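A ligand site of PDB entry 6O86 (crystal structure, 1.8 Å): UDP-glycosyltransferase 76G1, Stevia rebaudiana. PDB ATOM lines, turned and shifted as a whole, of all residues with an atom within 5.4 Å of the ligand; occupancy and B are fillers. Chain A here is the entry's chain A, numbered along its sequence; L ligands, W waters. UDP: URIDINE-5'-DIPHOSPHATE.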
ATOM      1  N   GLN A  23     -28.507 -24.874 -23.665  1.00  0.00           N
ATOM      2  CA  GLN A  23     -27.834 -23.651 -23.217  1.00  0.00           C
ATOM      3  C   GLN A  23     -28.770 -22.448 -23.234  1.00  0.00           C
ATOM      4  O   GLN A  23     -28.749 -21.630 -22.302  1.00  0.00           O
ATOM      5  CB  GLN A  23     -26.620 -23.384 -24.111  1.00  0.00           C
ATOM      6  CG  GLN A  23     -25.706 -22.272 -23.580  1.00  0.00           C
ATOM      7  CD  GLN A  23     -24.940 -22.713 -22.343  1.00  0.00           C
ATOM      8  OE1 GLN A  23     -23.865 -23.294 -22.452  1.00  0.00           O
ATOM      9  NE2 GLN A  23     -25.492 -22.425 -21.164  1.00  0.00           N
ATOM     10  N   GLY A  24     -29.581 -22.302 -24.285  1.00  0.00           N
ATOM     11  CA  GLY A  24     -30.458 -21.140 -24.391  1.00  0.00           C
ATOM     12  C   GLY A  24     -31.674 -21.201 -23.488  1.00  0.00           C
ATOM     13  O   GLY A  24     -32.428 -20.226 -23.430  1.00  0.00           O
ATOM     14  N   ASN A  27     -29.739 -20.911 -19.413  1.00  0.00           N
ATOM     15  CA  ASN A  27     -29.233 -19.576 -19.091  1.00  0.00           C
ATOM     16  C   ASN A  27     -30.311 -18.680 -18.507  1.00  0.00           C
ATOM     17  O   ASN A  27     -30.130 -18.169 -17.389  1.00  0.00           O
ATOM     18  CB  ASN A  27     -28.560 -18.970 -20.325  1.00  0.00           C
ATOM     19  CG  ASN A  27     -27.135 -19.482 -20.528  1.00  0.00           C
ATOM     20  OD1 ASN A  27     -26.667 -20.330 -19.776  1.00  0.00           O
ATOM     21  ND2 ASN A  27     -26.461 -18.977 -21.548  1.00  0.00           N
ATOM     22  N   ALA A 252     -25.013 -14.781 -17.863  1.00  0.00           N
ATOM     23  CA  ALA A 252     -25.227 -16.208 -17.691  1.00  0.00           C
ATOM     24  C   ALA A 252     -23.921 -16.990 -17.583  1.00  0.00           C
ATOM     25  O   ALA A 252     -23.910 -18.202 -17.824  1.00  0.00           O
ATOM     26  CB  ALA A 252     -26.077 -16.750 -18.840  1.00  0.00           C
ATOM     27  N   SER A 256     -22.699 -21.695 -18.044  1.00  0.00           N
ATOM     28  CA  SER A 256     -22.091 -22.167 -19.287  1.00  0.00           C
ATOM     29  C   SER A 256     -21.868 -23.679 -19.241  1.00  0.00           C
ATOM     30  O   SER A 256     -21.350 -24.225 -18.262  1.00  0.00           O
ATOM     31  CB  SER A 256     -20.763 -21.450 -19.521  1.00  0.00           C
ATOM     32  OG  SER A 256     -20.126 -21.936 -20.689  1.00  0.00           O
ATOM     33  N   HIS A 260     -14.878 -21.752 -20.852  1.00  0.00           N
ATOM     34  CA  HIS A 260     -14.618 -20.462 -21.462  1.00  0.00           C
ATOM     35  C   HIS A 260     -13.163 -20.356 -21.929  1.00  0.00           C
ATOM     36  O   HIS A 260     -12.237 -20.785 -21.227  1.00  0.00           O
ATOM     37  CB  HIS A 260     -14.885 -19.324 -20.470  1.00  0.00           C
ATOM     38  CG  HIS A 260     -16.328 -19.149 -20.135  1.00  0.00           C
ATOM     39  ND1 HIS A 260     -16.770 -19.011 -18.837  1.00  0.00           N
ATOM     40  CD2 HIS A 260     -17.422 -19.055 -20.920  1.00  0.00           C
ATOM     41  CE1 HIS A 260     -18.086 -18.871 -18.841  1.00  0.00           C
ATOM     42  NE2 HIS A 260     -18.505 -18.884 -20.096  1.00  0.00           N
ATOM     43  N   TYR A 278     -17.760  -9.294 -33.305  1.00  0.00           N
ATOM     44  CA  TYR A 278     -17.963 -10.564 -32.634  1.00  0.00           C
ATOM     45  C   TYR A 278     -18.919 -11.418 -33.461  1.00  0.00           C
ATOM     46  O   TYR A 278     -19.950 -10.917 -33.928  1.00  0.00           O
ATOM     47  CB  TYR A 278     -18.505 -10.342 -31.212  1.00  0.00           C
ATOM     48  CG  TYR A 278     -18.876 -11.614 -30.482  1.00  0.00           C
ATOM     49  CD1 TYR A 278     -17.896 -12.515 -30.074  1.00  0.00           C
ATOM     50  CD2 TYR A 278     -20.204 -11.902 -30.168  1.00  0.00           C
ATOM     51  CE1 TYR A 278     -18.224 -13.683 -29.415  1.00  0.00           C
ATOM     52  CE2 TYR A 278     -20.542 -13.076 -29.503  1.00  0.00           C
ATOM     53  CZ  TYR A 278     -19.556 -13.960 -29.127  1.00  0.00           C
ATOM     54  OH  TYR A 278     -19.876 -15.112 -28.456  1.00  0.00           O
ATOM     55  N   SER A 280     -20.872 -15.247 -33.657  1.00  0.00           N
ATOM     56  CA  SER A 280     -21.228 -16.490 -32.979  1.00  0.00           C
ATOM     57  C   SER A 280     -22.647 -16.876 -33.351  1.00  0.00           C
ATOM     58  O   SER A 280     -23.550 -16.039 -33.326  1.00  0.00           O
ATOM     59  CB  SER A 280     -21.119 -16.367 -31.454  1.00  0.00           C
ATOM     60  OG  SER A 280     -21.551 -17.577 -30.850  1.00  0.00           O
ATOM     61  N   PHE A 281     -22.857 -18.156 -33.646  1.00  0.00           N
ATOM     62  CA  PHE A 281     -24.164 -18.642 -34.048  1.00  0.00           C
ATOM     63  C   PHE A 281     -24.789 -19.582 -33.011  1.00  0.00           C
ATOM     64  O   PHE A 281     -25.538 -20.503 -33.365  1.00  0.00           O
ATOM     65  CB  PHE A 281     -24.075 -19.298 -35.428  1.00  0.00           C
ATOM     66  CG  PHE A 281     -23.509 -18.390 -36.485  1.00  0.00           C
ATOM     67  CD1 PHE A 281     -24.165 -17.204 -36.821  1.00  0.00           C
ATOM     68  CD2 PHE A 281     -22.331 -18.698 -37.142  1.00  0.00           C
ATOM     69  CE1 PHE A 281     -23.648 -16.362 -37.796  1.00  0.00           C
ATOM     70  CE2 PHE A 281     -21.802 -17.855 -38.112  1.00  0.00           C
ATOM     71  CZ  PHE A 281     -22.472 -16.679 -38.449  1.00  0.00           C
ATOM     72  N   GLY A 282     -24.524 -19.345 -31.736  1.00  0.00           N
ATOM     73  CA  GLY A 282     -25.276 -19.982 -30.665  1.00  0.00           C
ATOM     74  C   GLY A 282     -24.744 -21.346 -30.274  1.00  0.00           C
ATOM     75  O   GLY A 282     -23.596 -21.709 -30.537  1.00  0.00           O
ATOM     76  N   SER A 283     -25.609 -22.109 -29.603  1.00  0.00           N
ATOM     77  CA  SER A 283     -25.194 -23.337 -28.941  1.00  0.00           C
ATOM     78  C   SER A 283     -25.570 -24.614 -29.688  1.00  0.00           C
ATOM     79  O   SER A 283     -25.050 -25.685 -29.342  1.00  0.00           O
ATOM     80  CB  SER A 283     -25.795 -23.410 -27.525  1.00  0.00           C
ATOM     81  OG  SER A 283     -27.200 -23.565 -27.569  1.00  0.00           O
ATOM     82  N   THR A 284     -26.438 -24.545 -30.708  1.00  0.00           N
ATOM     83  CA  THR A 284     -26.838 -25.764 -31.411  1.00  0.00           C
ATOM     84  C   THR A 284     -26.722 -25.694 -32.923  1.00  0.00           C
ATOM     85  O   THR A 284     -26.868 -26.729 -33.576  1.00  0.00           O
ATOM     86  CB  THR A 284     -28.281 -26.159 -31.052  1.00  0.00           C
ATOM     87  OG1 THR A 284     -29.197 -25.228 -31.638  1.00  0.00           O
ATOM     88  CG2 THR A 284     -28.487 -26.169 -29.537  1.00  0.00           C
ATOM     89  N   VAL A 309     -16.485 -17.162 -32.664  1.00  0.00           N
ATOM     90  CA  VAL A 309     -16.746 -18.383 -31.907  1.00  0.00           C
ATOM     91  C   VAL A 309     -17.269 -19.428 -32.873  1.00  0.00           C
ATOM     92  O   VAL A 309     -18.313 -19.248 -33.505  1.00  0.00           O
ATOM     93  CB  VAL A 309     -17.758 -18.143 -30.771  1.00  0.00           C
ATOM     94  CG1 VAL A 309     -18.096 -19.476 -30.088  1.00  0.00           C
ATOM     95  CG2 VAL A 309     -17.215 -17.147 -29.760  1.00  0.00           C
ATOM     96  N   LYS A 337     -13.399 -21.552 -29.425  1.00  0.00           N
ATOM     97  CA  LYS A 337     -14.471 -22.533 -29.307  1.00  0.00           C
ATOM     98  C   LYS A 337     -15.661 -22.016 -28.498  1.00  0.00           C
ATOM     99  O   LYS A 337     -16.793 -22.434 -28.746  1.00  0.00           O
ATOM    100  CB  LYS A 337     -13.947 -23.817 -28.656  1.00  0.00           C
ATOM    101  CG  LYS A 337     -12.847 -24.502 -29.451  1.00  0.00           C
ATOM    102  CD  LYS A 337     -12.304 -25.723 -28.730  1.00  0.00           C
ATOM    103  CE  LYS A 337     -11.292 -26.465 -29.581  1.00  0.00           C
ATOM    104  NZ  LYS A 337     -10.639 -27.574 -28.824  1.00  0.00           N
ATOM    105  N   TRP A 338     -15.424 -21.105 -27.555  1.00  0.00           N
ATOM    106  CA  TRP A 338     -16.455 -20.689 -26.622  1.00  0.00           C
ATOM    107  C   TRP A 338     -15.922 -19.563 -25.740  1.00  0.00           C
ATOM    108  O   TRP A 338     -14.753 -19.606 -25.343  1.00  0.00           O
ATOM    109  CB  TRP A 338     -16.898 -21.884 -25.777  1.00  0.00           C
ATOM    110  CG  TRP A 338     -18.199 -21.703 -25.075  1.00  0.00           C
ATOM    111  CD1 TRP A 338     -18.397 -21.518 -23.736  1.00  0.00           C
ATOM    112  CD2 TRP A 338     -19.505 -21.743 -25.670  1.00  0.00           C
ATOM    113  NE1 TRP A 338     -19.743 -21.423 -23.466  1.00  0.00           N
ATOM    114  CE2 TRP A 338     -20.445 -21.561 -24.633  1.00  0.00           C
ATOM    115  CE3 TRP A 338     -19.966 -21.912 -26.983  1.00  0.00           C
ATOM    116  CZ2 TRP A 338     -21.819 -21.533 -24.869  1.00  0.00           C
ATOM    117  CZ3 TRP A 338     -21.329 -21.891 -27.209  1.00  0.00           C
ATOM    118  CH2 TRP A 338     -22.242 -21.699 -26.164  1.00  0.00           C
ATOM    119  N   VAL A 339     -16.754 -18.576 -25.446  1.00  0.00           N
ATOM    120  CA  VAL A 339     -16.353 -17.419 -24.637  1.00  0.00           C
ATOM    121  C   VAL A 339     -17.449 -17.087 -23.619  1.00  0.00           C
ATOM    122  O   VAL A 339     -18.567 -17.613 -23.713  1.00  0.00           O
ATOM    123  CB  VAL A 339     -16.066 -16.186 -25.502  1.00  0.00           C
ATOM    124  CG1 VAL A 339     -14.976 -16.498 -26.526  1.00  0.00           C
ATOM    125  CG2 VAL A 339     -17.339 -15.722 -26.200  1.00  0.00           C
ATOM    126  N   PRO A 340     -17.184 -16.222 -22.646  1.00  0.00           N
ATOM    127  CA  PRO A 340     -18.279 -15.655 -21.863  1.00  0.00           C
ATOM    128  C   PRO A 340     -18.922 -14.576 -22.705  1.00  0.00           C
ATOM    129  O   PRO A 340     -18.403 -13.462 -22.773  1.00  0.00           O
ATOM    130  CB  PRO A 340     -17.588 -15.093 -20.610  1.00  0.00           C
ATOM    131  CG  PRO A 340     -16.115 -15.537 -20.721  1.00  0.00           C
ATOM    132  CD  PRO A 340     -15.873 -15.743 -22.186  1.00  0.00           C
ATOM    133  N   GLN A 341     -20.021 -14.902 -23.409  1.00  0.00           N
ATOM    134  CA  GLN A 341     -20.440 -14.062 -24.537  1.00  0.00           C
ATOM    135  C   GLN A 341     -20.854 -12.665 -24.087  1.00  0.00           C
ATOM    136  O   GLN A 341     -20.414 -11.662 -24.678  1.00  0.00           O
ATOM    137  CB  GLN A 341     -21.565 -14.739 -25.307  1.00  0.00           C
ATOM    138  CG  GLN A 341     -22.208 -13.804 -26.334  1.00  0.00           C
ATOM    139  CD  GLN A 341     -23.077 -14.519 -27.335  1.00  0.00           C
ATOM    140  OE1 GLN A 341     -22.598 -15.335 -28.118  1.00  0.00           O
ATOM    141  NE2 GLN A 341     -24.371 -14.232 -27.304  1.00  0.00           N
ATOM    142  N   GLN A 342     -21.715 -12.553 -23.077  1.00  0.00           N
ATOM    143  CA  GLN A 342     -22.168 -11.210 -22.705  1.00  0.00           C
ATOM    144  C   GLN A 342     -21.009 -10.358 -22.216  1.00  0.00           C
ATOM    145  O   GLN A 342     -20.980  -9.137 -22.436  1.00  0.00           O
ATOM    146  CB  GLN A 342     -23.285 -11.264 -21.660  1.00  0.00           C
ATOM    147  CG  GLN A 342     -23.915  -9.894 -21.433  1.00  0.00           C
ATOM    148  CD  GLN A 342     -25.091  -9.906 -20.485  1.00  0.00           C
ATOM    149  OE1 GLN A 342     -25.641 -10.967 -20.170  1.00  0.00           O
ATOM    150  NE2 GLN A 342     -25.472  -8.730 -19.993  1.00  0.00           N
ATOM    151  N   HIS A 356     -26.731 -15.421 -34.979  1.00  0.00           N
ATOM    152  CA  HIS A 356     -27.757 -16.251 -35.590  1.00  0.00           C
ATOM    153  C   HIS A 356     -29.159 -15.856 -35.154  1.00  0.00           C
ATOM    154  O   HIS A 356     -30.127 -16.518 -35.556  1.00  0.00           O
ATOM    155  CB  HIS A 356     -27.498 -17.729 -35.271  1.00  0.00           C
ATOM    156  CG  HIS A 356     -27.902 -18.136 -33.883  1.00  0.00           C
ATOM    157  ND1 HIS A 356     -27.485 -17.458 -32.759  1.00  0.00           N
ATOM    158  CD2 HIS A 356     -28.655 -19.170 -33.437  1.00  0.00           C
ATOM    159  CE1 HIS A 356     -27.980 -18.042 -31.678  1.00  0.00           C
ATOM    160  NE2 HIS A 356     -28.690 -19.086 -32.067  1.00  0.00           N
ATOM    161  N   GLY A 358     -30.582 -16.019 -32.176  1.00  0.00           N
ATOM    162  CA  GLY A 358     -31.157 -16.617 -30.986  1.00  0.00           C
ATOM    163  C   GLY A 358     -31.565 -15.549 -30.000  1.00  0.00           C
ATOM    164  O   GLY A 358     -30.963 -14.465 -29.940  1.00  0.00           O
ATOM    165  N   TRP A 359     -32.622 -15.820 -29.228  1.00  0.00           N
ATOM    166  CA  TRP A 359     -33.198 -14.741 -28.418  1.00  0.00           C
ATOM    167  C   TRP A 359     -32.251 -14.317 -27.297  1.00  0.00           C
ATOM    168  O   TRP A 359     -32.144 -13.109 -27.023  1.00  0.00           O
ATOM    169  CB  TRP A 359     -34.559 -15.139 -27.849  1.00  0.00           C
ATOM    170  CG  TRP A 359     -35.212 -14.000 -27.102  1.00  0.00           C
ATOM    171  CD1 TRP A 359     -35.479 -13.929 -25.768  1.00  0.00           C
ATOM    172  CD2 TRP A 359     -35.629 -12.734 -27.662  1.00  0.00           C
ATOM    173  NE1 TRP A 359     -36.058 -12.720 -25.463  1.00  0.00           N
ATOM    174  CE2 TRP A 359     -36.157 -11.967 -26.596  1.00  0.00           C
ATOM    175  CE3 TRP A 359     -35.607 -12.184 -28.949  1.00  0.00           C
ATOM    176  CZ2 TRP A 359     -36.666 -10.681 -26.790  1.00  0.00           C
ATOM    177  CZ3 TRP A 359     -36.127 -10.914 -29.132  1.00  0.00           C
ATOM    178  CH2 TRP A 359     -36.647 -10.172 -28.047  1.00  0.00           C
ATOM    179  N   ASN A 360     -31.570 -15.247 -26.624  1.00  0.00           N
ATOM    180  CA  ASN A 360     -30.640 -14.802 -25.585  1.00  0.00           C
ATOM    181  C   ASN A 360     -29.547 -13.936 -26.174  1.00  0.00           C
ATOM    182  O   ASN A 360     -29.219 -12.871 -25.633  1.00  0.00           O
ATOM    183  CB  ASN A 360     -30.016 -15.991 -24.841  1.00  0.00           C
ATOM    184  CG  ASN A 360     -31.043 -16.799 -24.083  1.00  0.00           C
ATOM    185  OD1 ASN A 360     -31.519 -16.407 -23.013  1.00  0.00           O
ATOM    186  ND2 ASN A 360     -31.403 -17.957 -24.642  1.00  0.00           N
ATOM    187  N   SER A 361     -28.945 -14.371 -27.291  1.00  0.00           N
ATOM    188  CA  SER A 361     -27.879 -13.585 -27.895  1.00  0.00           C
ATOM    189  C   SER A 361     -28.375 -12.217 -28.313  1.00  0.00           C
ATOM    190  O   SER A 361     -27.679 -11.200 -28.126  1.00  0.00           O
ATOM    191  CB  SER A 361     -27.271 -14.324 -29.087  1.00  0.00           C
ATOM    192  OG  SER A 361     -26.524 -15.473 -28.666  1.00  0.00           O
ATOM    193  N   THR A 362     -29.579 -12.153 -28.889  1.00  0.00           N
ATOM    194  CA  THR A 362     -30.128 -10.886 -29.348  1.00  0.00           C
ATOM    195  C   THR A 362     -30.368  -9.940 -28.186  1.00  0.00           C
ATOM    196  O   THR A 362     -30.005  -8.755 -28.229  1.00  0.00           O
ATOM    197  CB  THR A 362     -31.440 -11.124 -30.127  1.00  0.00           C
ATOM    198  OG1 THR A 362     -31.192 -11.998 -31.229  1.00  0.00           O
ATOM    199  CG2 THR A 362     -32.007  -9.819 -30.652  1.00  0.00           C
ATOM    200  N   GLU A 364     -28.966 -10.116 -25.181  1.00  0.00           N
ATOM    201  CA  GLU A 364     -27.675  -9.739 -24.612  1.00  0.00           C
ATOM    202  C   GLU A 364     -27.078  -8.577 -25.381  1.00  0.00           C
ATOM    203  O   GLU A 364     -26.597  -7.592 -24.790  1.00  0.00           O
ATOM    204  CB  GLU A 364     -26.731 -10.930 -24.615  1.00  0.00           C
ATOM    205  CG  GLU A 364     -27.087 -12.017 -23.584  1.00  0.00           C
ATOM    206  CD  GLU A 364     -26.549 -13.372 -23.953  1.00  0.00           C
ATOM    207  OE1 GLU A 364     -25.624 -13.444 -24.785  1.00  0.00           O
ATOM    208  OE2 GLU A 364     -27.060 -14.386 -23.408  1.00  0.00           O
ATOM    209  N   GLN A 381     -35.707 -17.520 -34.991  1.00  0.00           N
ATOM    210  CA  GLN A 381     -34.572 -16.678 -35.380  1.00  0.00           C
ATOM    211  C   GLN A 381     -34.903 -15.719 -36.512  1.00  0.00           C
ATOM    212  O   GLN A 381     -34.571 -14.517 -36.387  1.00  0.00           O
ATOM    213  CB  GLN A 381     -33.378 -17.582 -35.709  1.00  0.00           C
ATOM    214  CG  GLN A 381     -32.852 -18.302 -34.455  1.00  0.00           C
ATOM    215  CD  GLN A 381     -31.952 -19.477 -34.770  1.00  0.00           C
ATOM    216  OE1 GLN A 381     -31.442 -19.613 -35.877  1.00  0.00           O
ATOM    217  NE2 GLN A 381     -31.758 -20.356 -33.776  1.00  0.00           N
HETATM  218  N1  UDP L   1     -22.963 -18.301 -25.439  1.00  0.00           N
HETATM  219  C2  UDP L   1     -21.845 -18.215 -24.645  1.00  0.00           C
HETATM  220  N3  UDP L   1     -20.603 -18.323 -25.213  1.00  0.00           N
HETATM  221  C4  UDP L   1     -20.474 -18.506 -26.570  1.00  0.00           C
HETATM  222  C5  UDP L   1     -21.594 -18.587 -27.377  1.00  0.00           C
HETATM  223  C6  UDP L   1     -22.851 -18.427 -26.800  1.00  0.00           C
HETATM  224  O2  UDP L   1     -21.946 -18.049 -23.431  1.00  0.00           O
HETATM  225  O4  UDP L   1     -19.341 -18.591 -27.055  1.00  0.00           O
HETATM  226  C1' UDP L   1     -24.289 -18.191 -24.825  1.00  0.00           C
HETATM  227  C2' UDP L   1     -24.965 -16.886 -25.200  1.00  0.00           C
HETATM  228  O2' UDP L   1     -24.477 -15.797 -24.435  1.00  0.00           O
HETATM  229  C3' UDP L   1     -26.429 -17.236 -24.990  1.00  0.00           C
HETATM  230  C4' UDP L   1     -26.478 -18.741 -25.283  1.00  0.00           C
HETATM  231  O4' UDP L   1     -25.145 -19.213 -25.290  1.00  0.00           O
HETATM  232  O3' UDP L   1     -26.855 -16.949 -23.678  1.00  0.00           O
HETATM  233  C5' UDP L   1     -27.103 -19.042 -26.648  1.00  0.00           C
HETATM  234  O5' UDP L   1     -28.490 -18.839 -26.590  1.00  0.00           O
HETATM  235  PA  UDP L   1     -29.291 -18.270 -27.853  1.00  0.00           P
HETATM  236  O1A UDP L   1     -28.646 -17.045 -28.378  1.00  0.00           O
HETATM  237  O2A UDP L   1     -30.686 -18.044 -27.443  1.00  0.00           O
HETATM  238  O3A UDP L   1     -29.140 -19.324 -29.062  1.00  0.00           O
HETATM  239  PB  UDP L   1     -29.331 -20.934 -29.033  1.00  0.00           P
HETATM  240  O1B UDP L   1     -28.091 -21.569 -28.564  1.00  0.00           O
HETATM  241  O2B UDP L   1     -29.575 -21.303 -30.437  1.00  0.00           O
HETATM  242  O3B UDP L   1     -30.477 -21.277 -28.159  1.00  0.00           O
HETATM  243  O   HOH W   1     -24.098 -17.028 -29.673  1.00  0.00           O
HETATM  244  O   HOH W   2     -27.601 -22.241 -32.015  1.00  0.00           O
HETATM  245  O   HOH W   3     -21.033 -18.129 -20.932  1.00  0.00           O
HETATM  246  O   HOH W   4     -30.647 -23.486 -26.576  1.00  0.00           O
HETATM  247  O   HOH W   5     -33.315 -19.850 -27.680  1.00  0.00           O
HETATM  248  O   HOH W   6     -30.919 -23.563 -30.564  1.00  0.00           O
HETATM  249  O   HOH W   7     -23.528 -14.757 -21.990  1.00  0.00           O
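Water W6 bridges the side-chain hydroxyl (OG1) of Thr 284 (2.6 Å) and an oxygen (O2B) of the ligand (2.6 Å).
Water W3 lies within hydrogen-bond range of O2 of the ligand and NE2 of His 260.
Water W2 lies within hydrogen-bond range of O2B of the ligand, N of Thr 284, O of Phe 281, N of Ser 283 and NE2 of His 356.
Water W4 bridges an oxygen (O3B) of the ligand (2.7 Å) and the backbone NH of Gly 24 (2.8 Å).
Water W7 lies within hydrogen-bond range of O2' of the ligand (2.8 Å) and N of Gln 342 (3.1 Å).
Water W1 lies within hydrogen-bond range of the side-chain amide oxygen of Gln 341 (2.7 Å), the side-chain hydroxyl of Ser 280 (2.9 Å), the side-chain hydroxyl of Ser 361 (3.1 Å) and the backbone NH of Gly 282 (3.1 Å).
O1B of the ligand lies within hydrogen-bond range of N of Ser 283 (2.7 Å).
The side-chain hydroxyl (OG) of Ser 283 lies within hydrogen-bond range of an oxygen (O1B) of the ligand (2.4 Å).
OE2 of Glu 364 sits at hydrogen-bond distance from O3' of the ligand (2.6 Å).
The backbone NH of Val 339 sits at hydrogen-bond distance from an oxygen (O4) of the ligand, at 3.0 Å.
The backbone carbonyl oxygen (O) of Val 339 lies within hydrogen-bond range of a nitrogen (N3) of the ligand (2.6 Å).
O1A of the ligand is in hydrogen-bond range of N of Ser 361, at 2.9 Å.
The side-chain hydroxyl (OG) of Ser 361 is in hydrogen-bond range of an oxygen (O1A) of the ligand (2.7 Å).
A ring nitrogen (NE2) of His 356 sits at hydrogen-bond distance from an oxygen (O2B) of the ligand (2.9 Å).
The backbone NH (N) of Asn 360 sits at hydrogen-bond distance from an oxygen (O2A) of the ligand (3.0 Å).
An oxygen (O2A) of the ligand sits at hydrogen-bond distance from the side-chain amide nitrogen (ND2) of Asn 360 (2.9 Å).
An oxygen (O3') of the ligand is in hydrogen-bond range of the side-chain amide nitrogen (ND2) of Asn 27 (3.0 Å).
O2' of the ligand sits close to NE2 of Gln 341.
O2A of the ligand lies within hydrogen-bond range of N of Trp 359, 3.4 Å away.
CG of Gln 23 touches O4' of the ligand (3.5 Å).
Gly 24 touches the ligand (CA to O5', 3.7 Å).
OH of Tyr 278 touches O4 of the ligand, 3.8 Å away.
Ser 280 touches the ligand (OG to C5, 3.6 Å).
C of Gly 282 touches O1B of the ligand (3.8 Å).
Val 309 touches the ligand.
CE2 of Trp 338 touches N3 of the ligand, at 3.3 Å.
Gly 358 touches the ligand.
Of the 27 residues printed, 17 come within 4 Å of the ligand.
The nearest printed residue that does not touch the ligand is Thr 284 (4.02 Å).
The side-chain carboxylate of Glu 364 is in hydrogen-bond range of the side-chain amide nitrogen of Gln 341 (2.9 Å).
The side-chain hydroxyl (OG) of Ser 361 sits at hydrogen-bond distance from the side-chain amide nitrogen (NE2) of Gln 341.
The backbone carbonyl oxygen of His 356 lies close to the side-chain amide oxygen of Gln 381 (3.4 Å).
ND2 of Asn 360 lies within hydrogen-bond range of O of Gly 24, at 2.8 Å.
The side-chain amide oxygen (OD1) of Asn 27 sits at hydrogen-bond distance from the side-chain amide nitrogen (NE2) of Gln 23 (2.8 Å).
The side-chain amide oxygen (OE1) of Gln 341 is in hydrogen-bond range of the side-chain hydroxyl (OH) of Tyr 278, 2.8 Å away.
NE1 of Trp 338 is in hydrogen-bond range of OG of Ser 256.
The backbone carbonyl oxygen (O) of Gly 358 sits at hydrogen-bond distance from the side-chain hydroxyl (OG1) of Thr 362.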
